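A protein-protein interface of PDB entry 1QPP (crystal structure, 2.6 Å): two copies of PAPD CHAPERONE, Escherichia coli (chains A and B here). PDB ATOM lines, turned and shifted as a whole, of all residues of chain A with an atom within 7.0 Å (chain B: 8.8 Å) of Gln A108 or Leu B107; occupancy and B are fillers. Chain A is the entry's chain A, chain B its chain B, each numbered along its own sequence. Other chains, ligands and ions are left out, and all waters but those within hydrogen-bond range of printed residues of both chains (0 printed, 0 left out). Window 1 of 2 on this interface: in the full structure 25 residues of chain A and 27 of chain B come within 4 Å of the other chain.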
ATOM      1  N   GLN A  34     -20.975  -2.842 -20.404  1.00  0.00           N
ATOM      2  CA  GLN A  34     -22.350  -3.112 -20.781  1.00  0.00           C
ATOM      3  C   GLN A  34     -23.280  -2.108 -20.108  1.00  0.00           C
ATOM      4  O   GLN A  34     -23.184  -1.974 -18.887  1.00  0.00           O
ATOM      5  CB  GLN A  34     -22.842  -4.503 -20.372  1.00  0.00           C
ATOM      6  CG  GLN A  34     -22.088  -5.675 -20.934  1.00  0.00           C
ATOM      7  CD  GLN A  34     -22.332  -6.953 -20.172  1.00  0.00           C
ATOM      8  OE1 GLN A  34     -23.438  -7.196 -19.695  1.00  0.00           O
ATOM      9  NE2 GLN A  34     -21.356  -7.831 -19.999  1.00  0.00           N
ATOM     10  N   TRP A  36     -27.498  -1.043 -19.399  1.00  0.00           N
ATOM     11  CA  TRP A  36     -28.907  -1.399 -19.654  1.00  0.00           C
ATOM     12  C   TRP A  36     -29.817  -0.685 -18.669  1.00  0.00           C
ATOM     13  O   TRP A  36     -29.347  -0.219 -17.635  1.00  0.00           O
ATOM     14  CB  TRP A  36     -29.107  -2.915 -19.703  1.00  0.00           C
ATOM     15  CG  TRP A  36     -28.942  -3.613 -18.389  1.00  0.00           C
ATOM     16  CD1 TRP A  36     -29.931  -3.924 -17.487  1.00  0.00           C
ATOM     17  CD2 TRP A  36     -27.720  -4.114 -17.846  1.00  0.00           C
ATOM     18  NE1 TRP A  36     -29.379  -4.583 -16.403  1.00  0.00           N
ATOM     19  CE2 TRP A  36     -28.032  -4.719 -16.602  1.00  0.00           C
ATOM     20  CE3 TRP A  36     -26.400  -4.109 -18.260  1.00  0.00           C
ATOM     21  CZ2 TRP A  36     -27.066  -5.275 -15.756  1.00  0.00           C
ATOM     22  CZ3 TRP A  36     -25.418  -4.640 -17.464  1.00  0.00           C
ATOM     23  CH2 TRP A  36     -25.762  -5.227 -16.230  1.00  0.00           C
ATOM     24  N   GLU A  38     -33.402  -0.657 -16.226  1.00  0.00           N
ATOM     25  CA  GLU A  38     -34.366  -1.472 -15.492  1.00  0.00           C
ATOM     26  C   GLU A  38     -35.528  -0.601 -15.013  1.00  0.00           C
ATOM     27  O   GLU A  38     -35.363   0.625 -14.970  1.00  0.00           O
ATOM     28  CB  GLU A  38     -33.733  -2.234 -14.337  1.00  0.00           C
ATOM     29  CG  GLU A  38     -32.822  -3.389 -14.698  1.00  0.00           C
ATOM     30  CD  GLU A  38     -31.979  -3.877 -13.544  1.00  0.00           C
ATOM     31  OE1 GLU A  38     -32.005  -3.329 -12.411  1.00  0.00           O
ATOM     32  OE2 GLU A  38     -31.234  -4.874 -13.702  1.00  0.00           O
ATOM     33  N   ASN A  89     -28.019   0.776 -15.469  1.00  0.00           N
ATOM     34  CA  ASN A  89     -27.109  -0.282 -15.054  1.00  0.00           C
ATOM     35  C   ASN A  89     -25.797  -0.226 -15.823  1.00  0.00           C
ATOM     36  O   ASN A  89     -25.822   0.124 -17.009  1.00  0.00           O
ATOM     37  CB  ASN A  89     -27.758  -1.671 -15.279  1.00  0.00           C
ATOM     38  CG  ASN A  89     -28.850  -1.956 -14.251  1.00  0.00           C
ATOM     39  OD1 ASN A  89     -28.618  -2.507 -13.175  1.00  0.00           O
ATOM     40  ND2 ASN A  89     -30.072  -1.504 -14.540  1.00  0.00           N
ATOM     41  N   LEU A  90     -24.673  -0.612 -15.220  1.00  0.00           N
ATOM     42  CA  LEU A  90     -23.372  -0.637 -15.868  1.00  0.00           C
ATOM     43  C   LEU A  90     -22.459  -1.770 -15.411  1.00  0.00           C
ATOM     44  O   LEU A  90     -22.158  -1.867 -14.224  1.00  0.00           O
ATOM     45  CB  LEU A  90     -22.619   0.697 -15.613  1.00  0.00           C
ATOM     46  CG  LEU A  90     -21.345   0.919 -16.441  1.00  0.00           C
ATOM     47  CD1 LEU A  90     -21.601   1.192 -17.914  1.00  0.00           C
ATOM     48  CD2 LEU A  90     -20.630   2.129 -15.836  1.00  0.00           C
ATOM     49  N   ARG A  91     -22.000  -2.613 -16.326  1.00  0.00           N
ATOM     50  CA  ARG A  91     -21.096  -3.703 -15.951  1.00  0.00           C
ATOM     51  C   ARG A  91     -19.793  -3.580 -16.764  1.00  0.00           C
ATOM     52  O   ARG A  91     -19.767  -3.360 -17.980  1.00  0.00           O
ATOM     53  CB  ARG A  91     -21.704  -5.105 -16.132  1.00  0.00           C
ATOM     54  CG  ARG A  91     -20.825  -6.189 -15.556  1.00  0.00           C
ATOM     55  CD  ARG A  91     -21.047  -7.623 -16.001  1.00  0.00           C
ATOM     56  NE  ARG A  91     -22.352  -8.160 -15.632  1.00  0.00           N
ATOM     57  CZ  ARG A  91     -23.171  -8.761 -16.490  1.00  0.00           C
ATOM     58  NH1 ARG A  91     -22.744  -8.903 -17.751  1.00  0.00           N
ATOM     59  NH2 ARG A  91     -24.362  -9.214 -16.105  1.00  0.00           N
ATOM     60  N   GLU A  92     -18.685  -3.684 -16.049  1.00  0.00           N
ATOM     61  CA  GLU A  92     -17.376  -3.644 -16.674  1.00  0.00           C
ATOM     62  C   GLU A  92     -16.793  -5.056 -16.796  1.00  0.00           C
ATOM     63  O   GLU A  92     -16.625  -5.750 -15.779  1.00  0.00           O
ATOM     64  CB  GLU A  92     -16.462  -2.729 -15.871  1.00  0.00           C
ATOM     65  CG  GLU A  92     -16.335  -3.170 -14.422  1.00  0.00           C
ATOM     66  CD  GLU A  92     -15.060  -2.703 -13.761  1.00  0.00           C
ATOM     67  OE1 GLU A  92     -14.935  -1.480 -13.555  1.00  0.00           O
ATOM     68  OE2 GLU A  92     -14.213  -3.560 -13.459  1.00  0.00           O
ATOM     69  N   ALA A 106     -16.193  -9.727 -13.324  1.00  0.00           N
ATOM     70  CA  ALA A 106     -16.978  -8.595 -13.749  1.00  0.00           C
ATOM     71  C   ALA A 106     -17.640  -7.881 -12.578  1.00  0.00           C
ATOM     72  O   ALA A 106     -18.130  -8.538 -11.665  1.00  0.00           O
ATOM     73  CB  ALA A 106     -18.106  -9.078 -14.670  1.00  0.00           C
ATOM     74  N   LEU A 107     -17.684  -6.561 -12.592  1.00  0.00           N
ATOM     75  CA  LEU A 107     -18.370  -5.809 -11.564  1.00  0.00           C
ATOM     76  C   LEU A 107     -19.423  -4.924 -12.257  1.00  0.00           C
ATOM     77  O   LEU A 107     -19.260  -4.449 -13.367  1.00  0.00           O
ATOM     78  CB  LEU A 107     -17.493  -4.958 -10.668  1.00  0.00           C
ATOM     79  CG  LEU A 107     -16.359  -5.611  -9.884  1.00  0.00           C
ATOM     80  CD1 LEU A 107     -15.440  -4.501  -9.327  1.00  0.00           C
ATOM     81  CD2 LEU A 107     -16.787  -6.526  -8.757  1.00  0.00           C
ATOM     82  N   GLN A 108     -20.564  -4.772 -11.574  1.00  0.00           N
ATOM     83  CA  GLN A 108     -21.616  -3.929 -12.093  1.00  0.00           C
ATOM     84  C   GLN A 108     -22.112  -3.014 -10.977  1.00  0.00           C
ATOM     85  O   GLN A 108     -21.931  -3.276  -9.785  1.00  0.00           O
ATOM     86  CB  GLN A 108     -22.813  -4.673 -12.697  1.00  0.00           C
ATOM     87  CG  GLN A 108     -23.887  -5.071 -11.723  1.00  0.00           C
ATOM     88  CD  GLN A 108     -25.112  -5.735 -12.311  1.00  0.00           C
ATOM     89  OE1 GLN A 108     -25.033  -6.950 -12.528  1.00  0.00           O
ATOM     90  NE2 GLN A 108     -26.222  -5.028 -12.538  1.00  0.00           N
ATOM     91  N   THR A 109     -22.782  -1.976 -11.453  1.00  0.00           N
ATOM     92  CA  THR A 109     -23.367  -1.027 -10.518  1.00  0.00           C
ATOM     93  C   THR A 109     -24.707  -0.622 -11.101  1.00  0.00           C
ATOM     94  O   THR A 109     -24.864  -0.730 -12.318  1.00  0.00           O
ATOM     95  CB  THR A 109     -22.479   0.214 -10.270  1.00  0.00           C
ATOM     96  OG1 THR A 109     -22.950   0.693  -8.990  1.00  0.00           O
ATOM     97  CG2 THR A 109     -22.569   1.305 -11.333  1.00  0.00           C
ATOM     98  N   LYS A 110     -25.600  -0.141 -10.262  1.00  0.00           N
ATOM     99  CA  LYS A 110     -26.830   0.425 -10.821  1.00  0.00           C
ATOM    100  C   LYS A 110     -26.997   1.736 -10.074  1.00  0.00           C
ATOM    101  O   LYS A 110     -26.642   1.853  -8.892  1.00  0.00           O
ATOM    102  CB  LYS A 110     -27.999  -0.514 -10.754  1.00  0.00           C
ATOM    103  CG  LYS A 110     -28.519  -0.868  -9.359  1.00  0.00           C
ATOM    104  CD  LYS A 110     -29.633  -1.912  -9.491  1.00  0.00           C
ATOM    105  CE  LYS A 110     -29.109  -3.229 -10.056  1.00  0.00           C
ATOM    106  NZ  LYS A 110     -30.235  -4.153 -10.340  1.00  0.00           N
ATOM    107  N   ALA B   1     -14.987  -2.819   0.714  1.00  0.00           N
ATOM    108  CA  ALA B   1     -14.906  -3.721  -0.480  1.00  0.00           C
ATOM    109  C   ALA B   1     -14.935  -5.185  -0.021  1.00  0.00           C
ATOM    110  O   ALA B   1     -14.011  -5.700   0.611  1.00  0.00           O
ATOM    111  CB  ALA B   1     -13.719  -3.500  -1.394  1.00  0.00           C
ATOM    112  N   VAL B   2     -16.037  -5.841  -0.380  1.00  0.00           N
ATOM    113  CA  VAL B   2     -16.199  -7.256  -0.044  1.00  0.00           C
ATOM    114  C   VAL B   2     -15.634  -8.091  -1.182  1.00  0.00           C
ATOM    115  O   VAL B   2     -15.797  -7.780  -2.364  1.00  0.00           O
ATOM    116  CB  VAL B   2     -17.655  -7.617   0.288  1.00  0.00           C
ATOM    117  CG1 VAL B   2     -17.714  -8.830   1.200  1.00  0.00           C
ATOM    118  CG2 VAL B   2     -18.303  -6.421   0.997  1.00  0.00           C
ATOM    119  N   TYR B  31     -19.402  -2.702   6.317  1.00  0.00           N
ATOM    120  CA  TYR B  31     -20.152  -2.919   5.066  1.00  0.00           C
ATOM    121  C   TYR B  31     -21.241  -3.978   5.210  1.00  0.00           C
ATOM    122  O   TYR B  31     -21.104  -4.896   6.013  1.00  0.00           O
ATOM    123  CB  TYR B  31     -19.220  -3.375   3.939  1.00  0.00           C
ATOM    124  CG  TYR B  31     -18.566  -2.315   3.097  1.00  0.00           C
ATOM    125  CD1 TYR B  31     -17.464  -1.616   3.595  1.00  0.00           C
ATOM    126  CD2 TYR B  31     -19.011  -1.980   1.834  1.00  0.00           C
ATOM    127  CE1 TYR B  31     -16.847  -0.613   2.887  1.00  0.00           C
ATOM    128  CE2 TYR B  31     -18.364  -1.006   1.098  1.00  0.00           C
ATOM    129  CZ  TYR B  31     -17.293  -0.321   1.620  1.00  0.00           C
ATOM    130  OH  TYR B  31     -16.677   0.691   0.899  1.00  0.00           O
ATOM    131  N   LEU B  32     -22.306  -3.865   4.442  1.00  0.00           N
ATOM    132  CA  LEU B  32     -23.328  -4.921   4.429  1.00  0.00           C
ATOM    133  C   LEU B  32     -23.046  -5.834   3.238  1.00  0.00           C
ATOM    134  O   LEU B  32     -22.539  -5.333   2.213  1.00  0.00           O
ATOM    135  CB  LEU B  32     -24.679  -4.270   4.292  1.00  0.00           C
ATOM    136  CG  LEU B  32     -25.140  -3.309   5.363  1.00  0.00           C
ATOM    137  CD1 LEU B  32     -26.541  -2.837   5.008  1.00  0.00           C
ATOM    138  CD2 LEU B  32     -25.099  -3.932   6.743  1.00  0.00           C
ATOM    139  N   ALA B  33     -23.287  -7.128   3.399  1.00  0.00           N
ATOM    140  CA  ALA B  33     -23.052  -8.049   2.256  1.00  0.00           C
ATOM    141  C   ALA B  33     -24.394  -8.688   1.938  1.00  0.00           C
ATOM    142  O   ALA B  33     -25.013  -9.296   2.811  1.00  0.00           O
ATOM    143  CB  ALA B  33     -21.957  -9.091   2.442  1.00  0.00           C
ATOM    144  N   GLN B  34     -24.898  -8.425   0.757  1.00  0.00           N
ATOM    145  CA  GLN B  34     -26.179  -8.971   0.320  1.00  0.00           C
ATOM    146  C   GLN B  34     -25.871 -10.120  -0.635  1.00  0.00           C
ATOM    147  O   GLN B  34     -25.051  -9.977  -1.559  1.00  0.00           O
ATOM    148  CB  GLN B  34     -26.984  -7.899  -0.363  1.00  0.00           C
ATOM    149  CG  GLN B  34     -28.484  -8.013  -0.192  1.00  0.00           C
ATOM    150  CD  GLN B  34     -29.257  -6.889  -0.838  1.00  0.00           C
ATOM    151  OE1 GLN B  34     -28.615  -6.030  -1.440  1.00  0.00           O
ATOM    152  NE2 GLN B  34     -30.585  -6.909  -0.737  1.00  0.00           N
ATOM    153  N   TRP B  36     -27.537 -13.680  -2.812  1.00  0.00           N
ATOM    154  CA  TRP B  36     -28.765 -14.243  -3.354  1.00  0.00           C
ATOM    155  C   TRP B  36     -28.440 -15.200  -4.487  1.00  0.00           C
ATOM    156  O   TRP B  36     -27.308 -15.205  -4.961  1.00  0.00           O
ATOM    157  CB  TRP B  36     -29.779 -13.189  -3.800  1.00  0.00           C
ATOM    158  CG  TRP B  36     -29.484 -12.359  -5.000  1.00  0.00           C
ATOM    159  CD1 TRP B  36     -29.868 -12.591  -6.285  1.00  0.00           C
ATOM    160  CD2 TRP B  36     -28.784 -11.094  -5.029  1.00  0.00           C
ATOM    161  NE1 TRP B  36     -29.455 -11.570  -7.109  1.00  0.00           N
ATOM    162  CE2 TRP B  36     -28.761 -10.651  -6.376  1.00  0.00           C
ATOM    163  CE3 TRP B  36     -28.150 -10.314  -4.056  1.00  0.00           C
ATOM    164  CZ2 TRP B  36     -28.139  -9.473  -6.764  1.00  0.00           C
ATOM    165  CZ3 TRP B  36     -27.515  -9.153  -4.443  1.00  0.00           C
ATOM    166  CH2 TRP B  36     -27.539  -8.741  -5.776  1.00  0.00           C
ATOM    167  N   GLU B  38     -29.477 -16.886  -8.396  1.00  0.00           N
ATOM    168  CA  GLU B  38     -30.226 -16.657  -9.620  1.00  0.00           C
ATOM    169  C   GLU B  38     -30.223 -17.948 -10.438  1.00  0.00           C
ATOM    170  O   GLU B  38     -29.293 -18.732 -10.214  1.00  0.00           O
ATOM    171  CB  GLU B  38     -29.728 -15.547 -10.509  1.00  0.00           C
ATOM    172  CG  GLU B  38     -30.068 -14.149 -10.006  1.00  0.00           C
ATOM    173  CD  GLU B  38     -29.255 -13.092 -10.714  1.00  0.00           C
ATOM    174  OE1 GLU B  38     -28.177 -13.384 -11.256  1.00  0.00           O
ATOM    175  OE2 GLU B  38     -29.681 -11.924 -10.760  1.00  0.00           O
ATOM    176  N   GLN B  42     -30.729 -15.836 -15.084  1.00  0.00           N
ATOM    177  CA  GLN B  42     -30.414 -14.681 -14.260  1.00  0.00           C
ATOM    178  C   GLN B  42     -31.645 -14.043 -13.620  1.00  0.00           C
ATOM    179  O   GLN B  42     -31.903 -12.831 -13.551  1.00  0.00           O
ATOM    180  CB  GLN B  42     -29.579 -13.676 -15.073  1.00  0.00           C
ATOM    181  CG  GLN B  42     -28.116 -14.023 -15.246  1.00  0.00           C
ATOM    182  CD  GLN B  42     -27.288 -13.002 -16.014  1.00  0.00           C
ATOM    183  OE1 GLN B  42     -26.999 -13.206 -17.196  1.00  0.00           O
ATOM    184  NE2 GLN B  42     -26.869 -11.901 -15.417  1.00  0.00           N
ATOM    185  N   ASN B  89     -24.832 -14.450  -6.313  1.00  0.00           N
ATOM    186  CA  ASN B  89     -24.683 -13.004  -6.373  1.00  0.00           C
ATOM    187  C   ASN B  89     -24.281 -12.382  -5.026  1.00  0.00           C
ATOM    188  O   ASN B  89     -24.673 -12.833  -3.937  1.00  0.00           O
ATOM    189  CB  ASN B  89     -25.963 -12.371  -6.874  1.00  0.00           C
ATOM    190  CG  ASN B  89     -26.254 -12.487  -8.343  1.00  0.00           C
ATOM    191  OD1 ASN B  89     -26.072 -11.546  -9.132  1.00  0.00           O
ATOM    192  ND2 ASN B  89     -26.734 -13.635  -8.808  1.00  0.00           N
ATOM    193  N   LEU B  90     -23.436 -11.321  -5.125  1.00  0.00           N
ATOM    194  CA  LEU B  90     -22.974 -10.610  -3.929  1.00  0.00           C
ATOM    195  C   LEU B  90     -23.020  -9.102  -4.194  1.00  0.00           C
ATOM    196  O   LEU B  90     -22.535  -8.605  -5.230  1.00  0.00           O
ATOM    197  CB  LEU B  90     -21.582 -11.032  -3.488  1.00  0.00           C
ATOM    198  CG  LEU B  90     -21.214 -11.141  -2.009  1.00  0.00           C
ATOM    199  CD1 LEU B  90     -19.705 -11.080  -1.799  1.00  0.00           C
ATOM    200  CD2 LEU B  90     -21.850 -10.059  -1.164  1.00  0.00           C
ATOM    201  N   ARG B  91     -23.647  -8.361  -3.295  1.00  0.00           N
ATOM    202  CA  ARG B  91     -23.757  -6.915  -3.431  1.00  0.00           C
ATOM    203  C   ARG B  91     -23.161  -6.272  -2.170  1.00  0.00           C
ATOM    204  O   ARG B  91     -23.668  -6.576  -1.084  1.00  0.00           O
ATOM    205  CB  ARG B  91     -25.186  -6.422  -3.632  1.00  0.00           C
ATOM    206  CG  ARG B  91     -25.360  -4.916  -3.682  1.00  0.00           C
ATOM    207  CD  ARG B  91     -26.813  -4.469  -3.733  1.00  0.00           C
ATOM    208  NE  ARG B  91     -27.462  -4.686  -4.989  1.00  0.00           N
ATOM    209  CZ  ARG B  91     -28.623  -5.172  -5.368  1.00  0.00           C
ATOM    210  NH1 ARG B  91     -29.597  -5.567  -4.559  1.00  0.00           N
ATOM    211  NH2 ARG B  91     -28.863  -5.235  -6.675  1.00  0.00           N
ATOM    212  N   GLU B  92     -22.105  -5.482  -2.311  1.00  0.00           N
ATOM    213  CA  GLU B  92     -21.554  -4.777  -1.150  1.00  0.00           C
ATOM    214  C   GLU B  92     -22.242  -3.429  -0.932  1.00  0.00           C
ATOM    215  O   GLU B  92     -22.470  -2.692  -1.896  1.00  0.00           O
ATOM    216  CB  GLU B  92     -20.060  -4.587  -1.355  1.00  0.00           C
ATOM    217  CG  GLU B  92     -19.725  -3.520  -2.392  1.00  0.00           C
ATOM    218  CD  GLU B  92     -18.419  -2.837  -2.075  1.00  0.00           C
ATOM    219  OE1 GLU B  92     -17.388  -3.538  -2.035  1.00  0.00           O
ATOM    220  OE2 GLU B  92     -18.421  -1.612  -1.855  1.00  0.00           O
ATOM    221  N   ILE B  93     -22.703  -3.140   0.295  1.00  0.00           N
ATOM    222  CA  ILE B  93     -23.426  -1.878   0.542  1.00  0.00           C
ATOM    223  C   ILE B  93     -22.667  -0.980   1.505  1.00  0.00           C
ATOM    224  O   ILE B  93     -22.464  -1.324   2.669  1.00  0.00           O
ATOM    225  CB  ILE B  93     -24.855  -2.131   1.072  1.00  0.00           C
ATOM    226  CG1 ILE B  93     -25.640  -3.119   0.210  1.00  0.00           C
ATOM    227  CG2 ILE B  93     -25.614  -0.800   1.168  1.00  0.00           C
ATOM    228  CD1 ILE B  93     -27.164  -3.068   0.218  1.00  0.00           C
ATOM    229  N   PRO B  94     -22.169   0.150   1.059  1.00  0.00           N
ATOM    230  CA  PRO B  94     -21.351   1.087   1.829  1.00  0.00           C
ATOM    231  C   PRO B  94     -22.134   1.895   2.844  1.00  0.00           C
ATOM    232  O   PRO B  94     -23.328   2.128   2.691  1.00  0.00           O
ATOM    233  CB  PRO B  94     -20.668   2.019   0.813  1.00  0.00           C
ATOM    234  CG  PRO B  94     -21.768   2.041  -0.245  1.00  0.00           C
ATOM    235  CD  PRO B  94     -22.308   0.615  -0.332  1.00  0.00           C
ATOM    236  N   LEU B 103     -16.449   5.062  -2.467  1.00  0.00           N
ATOM    237  CA  LEU B 103     -17.626   5.004  -3.330  1.00  0.00           C
ATOM    238  C   LEU B 103     -18.871   4.887  -2.440  1.00  0.00           C
ATOM    239  O   LEU B 103     -18.951   4.138  -1.483  1.00  0.00           O
ATOM    240  CB  LEU B 103     -17.632   3.912  -4.362  1.00  0.00           C
ATOM    241  CG  LEU B 103     -16.402   3.631  -5.209  1.00  0.00           C
ATOM    242  CD1 LEU B 103     -16.789   2.471  -6.134  1.00  0.00           C
ATOM    243  CD2 LEU B 103     -15.860   4.817  -5.999  1.00  0.00           C
ATOM    244  N   GLN B 104     -19.858   5.681  -2.784  1.00  0.00           N
ATOM    245  CA  GLN B 104     -21.096   5.825  -2.081  1.00  0.00           C
ATOM    246  C   GLN B 104     -22.220   5.219  -2.902  1.00  0.00           C
ATOM    247  O   GLN B 104     -23.334   5.723  -2.916  1.00  0.00           O
ATOM    248  CB  GLN B 104     -21.363   7.305  -1.775  1.00  0.00           C
ATOM    249  CG  GLN B 104     -20.468   7.869  -0.696  1.00  0.00           C
ATOM    250  CD  GLN B 104     -20.789   7.305   0.674  1.00  0.00           C
ATOM    251  OE1 GLN B 104     -21.603   7.907   1.420  1.00  0.00           O
ATOM    252  NE2 GLN B 104     -20.199   6.161   1.058  1.00  0.00           N
ATOM    253  N   ILE B 105     -21.923   4.117  -3.579  1.00  0.00           N
ATOM    254  CA  ILE B 105     -22.946   3.339  -4.261  1.00  0.00           C
ATOM    255  C   ILE B 105     -22.587   1.858  -4.103  1.00  0.00           C
ATOM    256  O   ILE B 105     -21.421   1.538  -3.871  1.00  0.00           O
ATOM    257  CB  ILE B 105     -23.038   3.656  -5.750  1.00  0.00           C
ATOM    258  CG1 ILE B 105     -21.638   3.943  -6.323  1.00  0.00           C
ATOM    259  CG2 ILE B 105     -23.997   4.822  -5.966  1.00  0.00           C
ATOM    260  CD1 ILE B 105     -21.473   3.344  -7.695  1.00  0.00           C
ATOM    261  N   ALA B 106     -23.586   0.997  -4.207  1.00  0.00           N
ATOM    262  CA  ALA B 106     -23.369  -0.433  -4.065  1.00  0.00           C
ATOM    263  C   ALA B 106     -22.763  -1.008  -5.334  1.00  0.00           C
ATOM    264  O   ALA B 106     -23.075  -0.658  -6.476  1.00  0.00           O
ATOM    265  CB  ALA B 106     -24.668  -1.094  -3.659  1.00  0.00           C
ATOM    266  N   LEU B 107     -21.858  -1.957  -5.170  1.00  0.00           N
ATOM    267  CA  LEU B 107     -21.249  -2.651  -6.294  1.00  0.00           C
ATOM    268  C   LEU B 107     -21.695  -4.114  -6.125  1.00  0.00           C
ATOM    269  O   LEU B 107     -21.999  -4.538  -5.004  1.00  0.00           O
ATOM    270  CB  LEU B 107     -19.742  -2.513  -6.342  1.00  0.00           C
ATOM    271  CG  LEU B 107     -19.152  -1.128  -6.661  1.00  0.00           C
ATOM    272  CD1 LEU B 107     -17.631  -1.145  -6.562  1.00  0.00           C
ATOM    273  CD2 LEU B 107     -19.533  -0.693  -8.078  1.00  0.00           C
ATOM    274  N   GLN B 108     -21.764  -4.844  -7.237  1.00  0.00           N
ATOM    275  CA  GLN B 108     -22.167  -6.240  -7.142  1.00  0.00           C
ATOM    276  C   GLN B 108     -21.435  -7.088  -8.174  1.00  0.00           C
ATOM    277  O   GLN B 108     -20.711  -6.610  -9.059  1.00  0.00           O
ATOM    278  CB  GLN B 108     -23.678  -6.369  -7.255  1.00  0.00           C
ATOM    279  CG  GLN B 108     -24.263  -6.225  -8.630  1.00  0.00           C
ATOM    280  CD  GLN B 108     -25.690  -6.745  -8.766  1.00  0.00           C
ATOM    281  OE1 GLN B 108     -26.578  -5.897  -8.842  1.00  0.00           O
ATOM    282  NE2 GLN B 108     -25.863  -8.071  -8.795  1.00  0.00           N
ATOM    283  N   THR B 109     -21.608  -8.384  -8.017  1.00  0.00           N
ATOM    284  CA  THR B 109     -20.980  -9.333  -8.921  1.00  0.00           C
ATOM    285  C   THR B 109     -21.736 -10.652  -8.840  1.00  0.00           C
ATOM    286  O   THR B 109     -22.504 -10.900  -7.908  1.00  0.00           O
ATOM    287  CB  THR B 109     -19.500  -9.526  -8.527  1.00  0.00           C
ATOM    288  OG1 THR B 109     -18.897 -10.328  -9.553  1.00  0.00           O
ATOM    289  CG2 THR B 109     -19.311 -10.222  -7.185  1.00  0.00           C
ATOM    290  N   LYS B 110     -21.543 -11.517  -9.812  1.00  0.00           N
ATOM    291  CA  LYS B 110     -22.118 -12.846  -9.775  1.00  0.00           C
ATOM    292  C   LYS B 110     -21.052 -13.795 -10.325  1.00  0.00           C
ATOM    293  O   LYS B 110     -20.441 -13.376 -11.302  1.00  0.00           O
ATOM    294  CB  LYS B 110     -23.414 -12.994 -10.551  1.00  0.00           C
ATOM    295  CG  LYS B 110     -23.338 -12.687 -12.018  1.00  0.00           C
ATOM    296  CD  LYS B 110     -24.696 -12.532 -12.660  1.00  0.00           C
ATOM    297  CE  LYS B 110     -25.527 -11.418 -12.053  1.00  0.00           C
ATOM    298  NZ  LYS B 110     -26.823 -11.328 -12.795  1.00  0.00           N
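The side-chain hydroxyl (OG1) of Thr B109 sits at hydrogen-bond distance from the backbone carbonyl oxygen (O) of Ala A106 (2.9 Å).
The backbone NH of Gln B108 lies within hydrogen-bond range of the backbone carbonyl oxygen of Gln A108 (3.0 Å).
The side-chain hydroxyl of Thr A109 is in hydrogen-bond range of the backbone carbonyl oxygen of Ala B106, 2.9 Å away.
Among the printed residues, merely in contact across the chains: Arg A91 with Gln B42 (3.7 Å), Leu A107 with Gln B108 (3.5 Å), Gln A108 with Leu B107 (3.6 Å), Thr A109 with Ile B105 (3.3 Å), Thr A109 with Leu B107 (3.8 Å), Lys A110 with Arg B91 (3.9 Å) and Lys A110 with Gln B108 (3.9 Å).
Asn A89 touches none of the printed residues of chain B.
Of the printed residues of chain B, Arg A91 touches Gln B42.
Of chain B, only Ile B105, Ala B106 and Leu B107 come within 4 Å of Thr A109.
Printed residues of chain B within 4 Å of Lys A110: Arg B91 and Gln B108.
Ile B93 touches none of the printed residues of chain A.
Of the printed residues of chain A, Ile B105 touches Thr A109 (3.3 Å).
Leu B107 touches two residues of chain A.
Printed residues of chain A within 4 Å of Thr B109: Ala A106.
The nearest residue of chain B that does not touch Gln A108 is Ala B106 (4.4 Å).
The nearest residue of chain A that does not touch Leu B107 is Leu A107 (4.9 Å).
The guanidinium group of Arg A91 sits at hydrogen-bond distance from the side-chain amide oxygen of Gln A34 (2.7 Å).
NZ of Lys A110 is in salt-bridge range of OE1 of Glu A38, 2.8 Å away.
O of Leu A90 lies within hydrogen-bond range of N of Thr A109 (2.8 Å).
O of Leu A107 sits at hydrogen-bond distance from N of Glu A92.
The backbone NH (N) of Arg B91 is in hydrogen-bond range of the backbone carbonyl oxygen (O) of Gln B34.
The backbone NH (N) of Glu B92 lies within hydrogen-bond range of the backbone carbonyl oxygen (O) of Leu B107 (2.9 Å).
Hydrophobic or aromatic side chains of chain B that line the printed part of chain A: Ile B105 and Leu B107.
Of the 12 printed residues of chain A, 6 touch a printed residue of chain B.
Printed residues of chain A that touch a printed residue of chain B: Arg A91, Ala A106, Leu A107, Gln A108, Thr A109 and Lys A110.
Hydrophobic or aromatic side chains of chain A within 4 Å of the printed part of chain B: Leu A107.
Along chain A the printed residues that touch a printed residue of chain B span positions 91 to 110.
Among the printed residues, 10 pairs touch across the chains.
Among the printed residues, no Asp or Glu carboxylate lies within 4 Å of a Lys or Arg side-chain nitrogen of the other chain.
Leu A107 touches Gln B108, and with the chains exchanged Gln A108 touches Leu B107.
Gln B108 touches its own counterpart, Gln A108.
Lys A110 touches Arg B91, but with the chains exchanged Arg A91 does not touch Lys B110 (4.6 Å).
Lys A110 touches Gln B108, but with the chains exchanged Gln A108 does not touch Lys B110 (4.5 Å).
Positions printed for both chains: 34, 36, 38, 89, 90, 91, 92, 106, 107, 108, 109 and 110.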
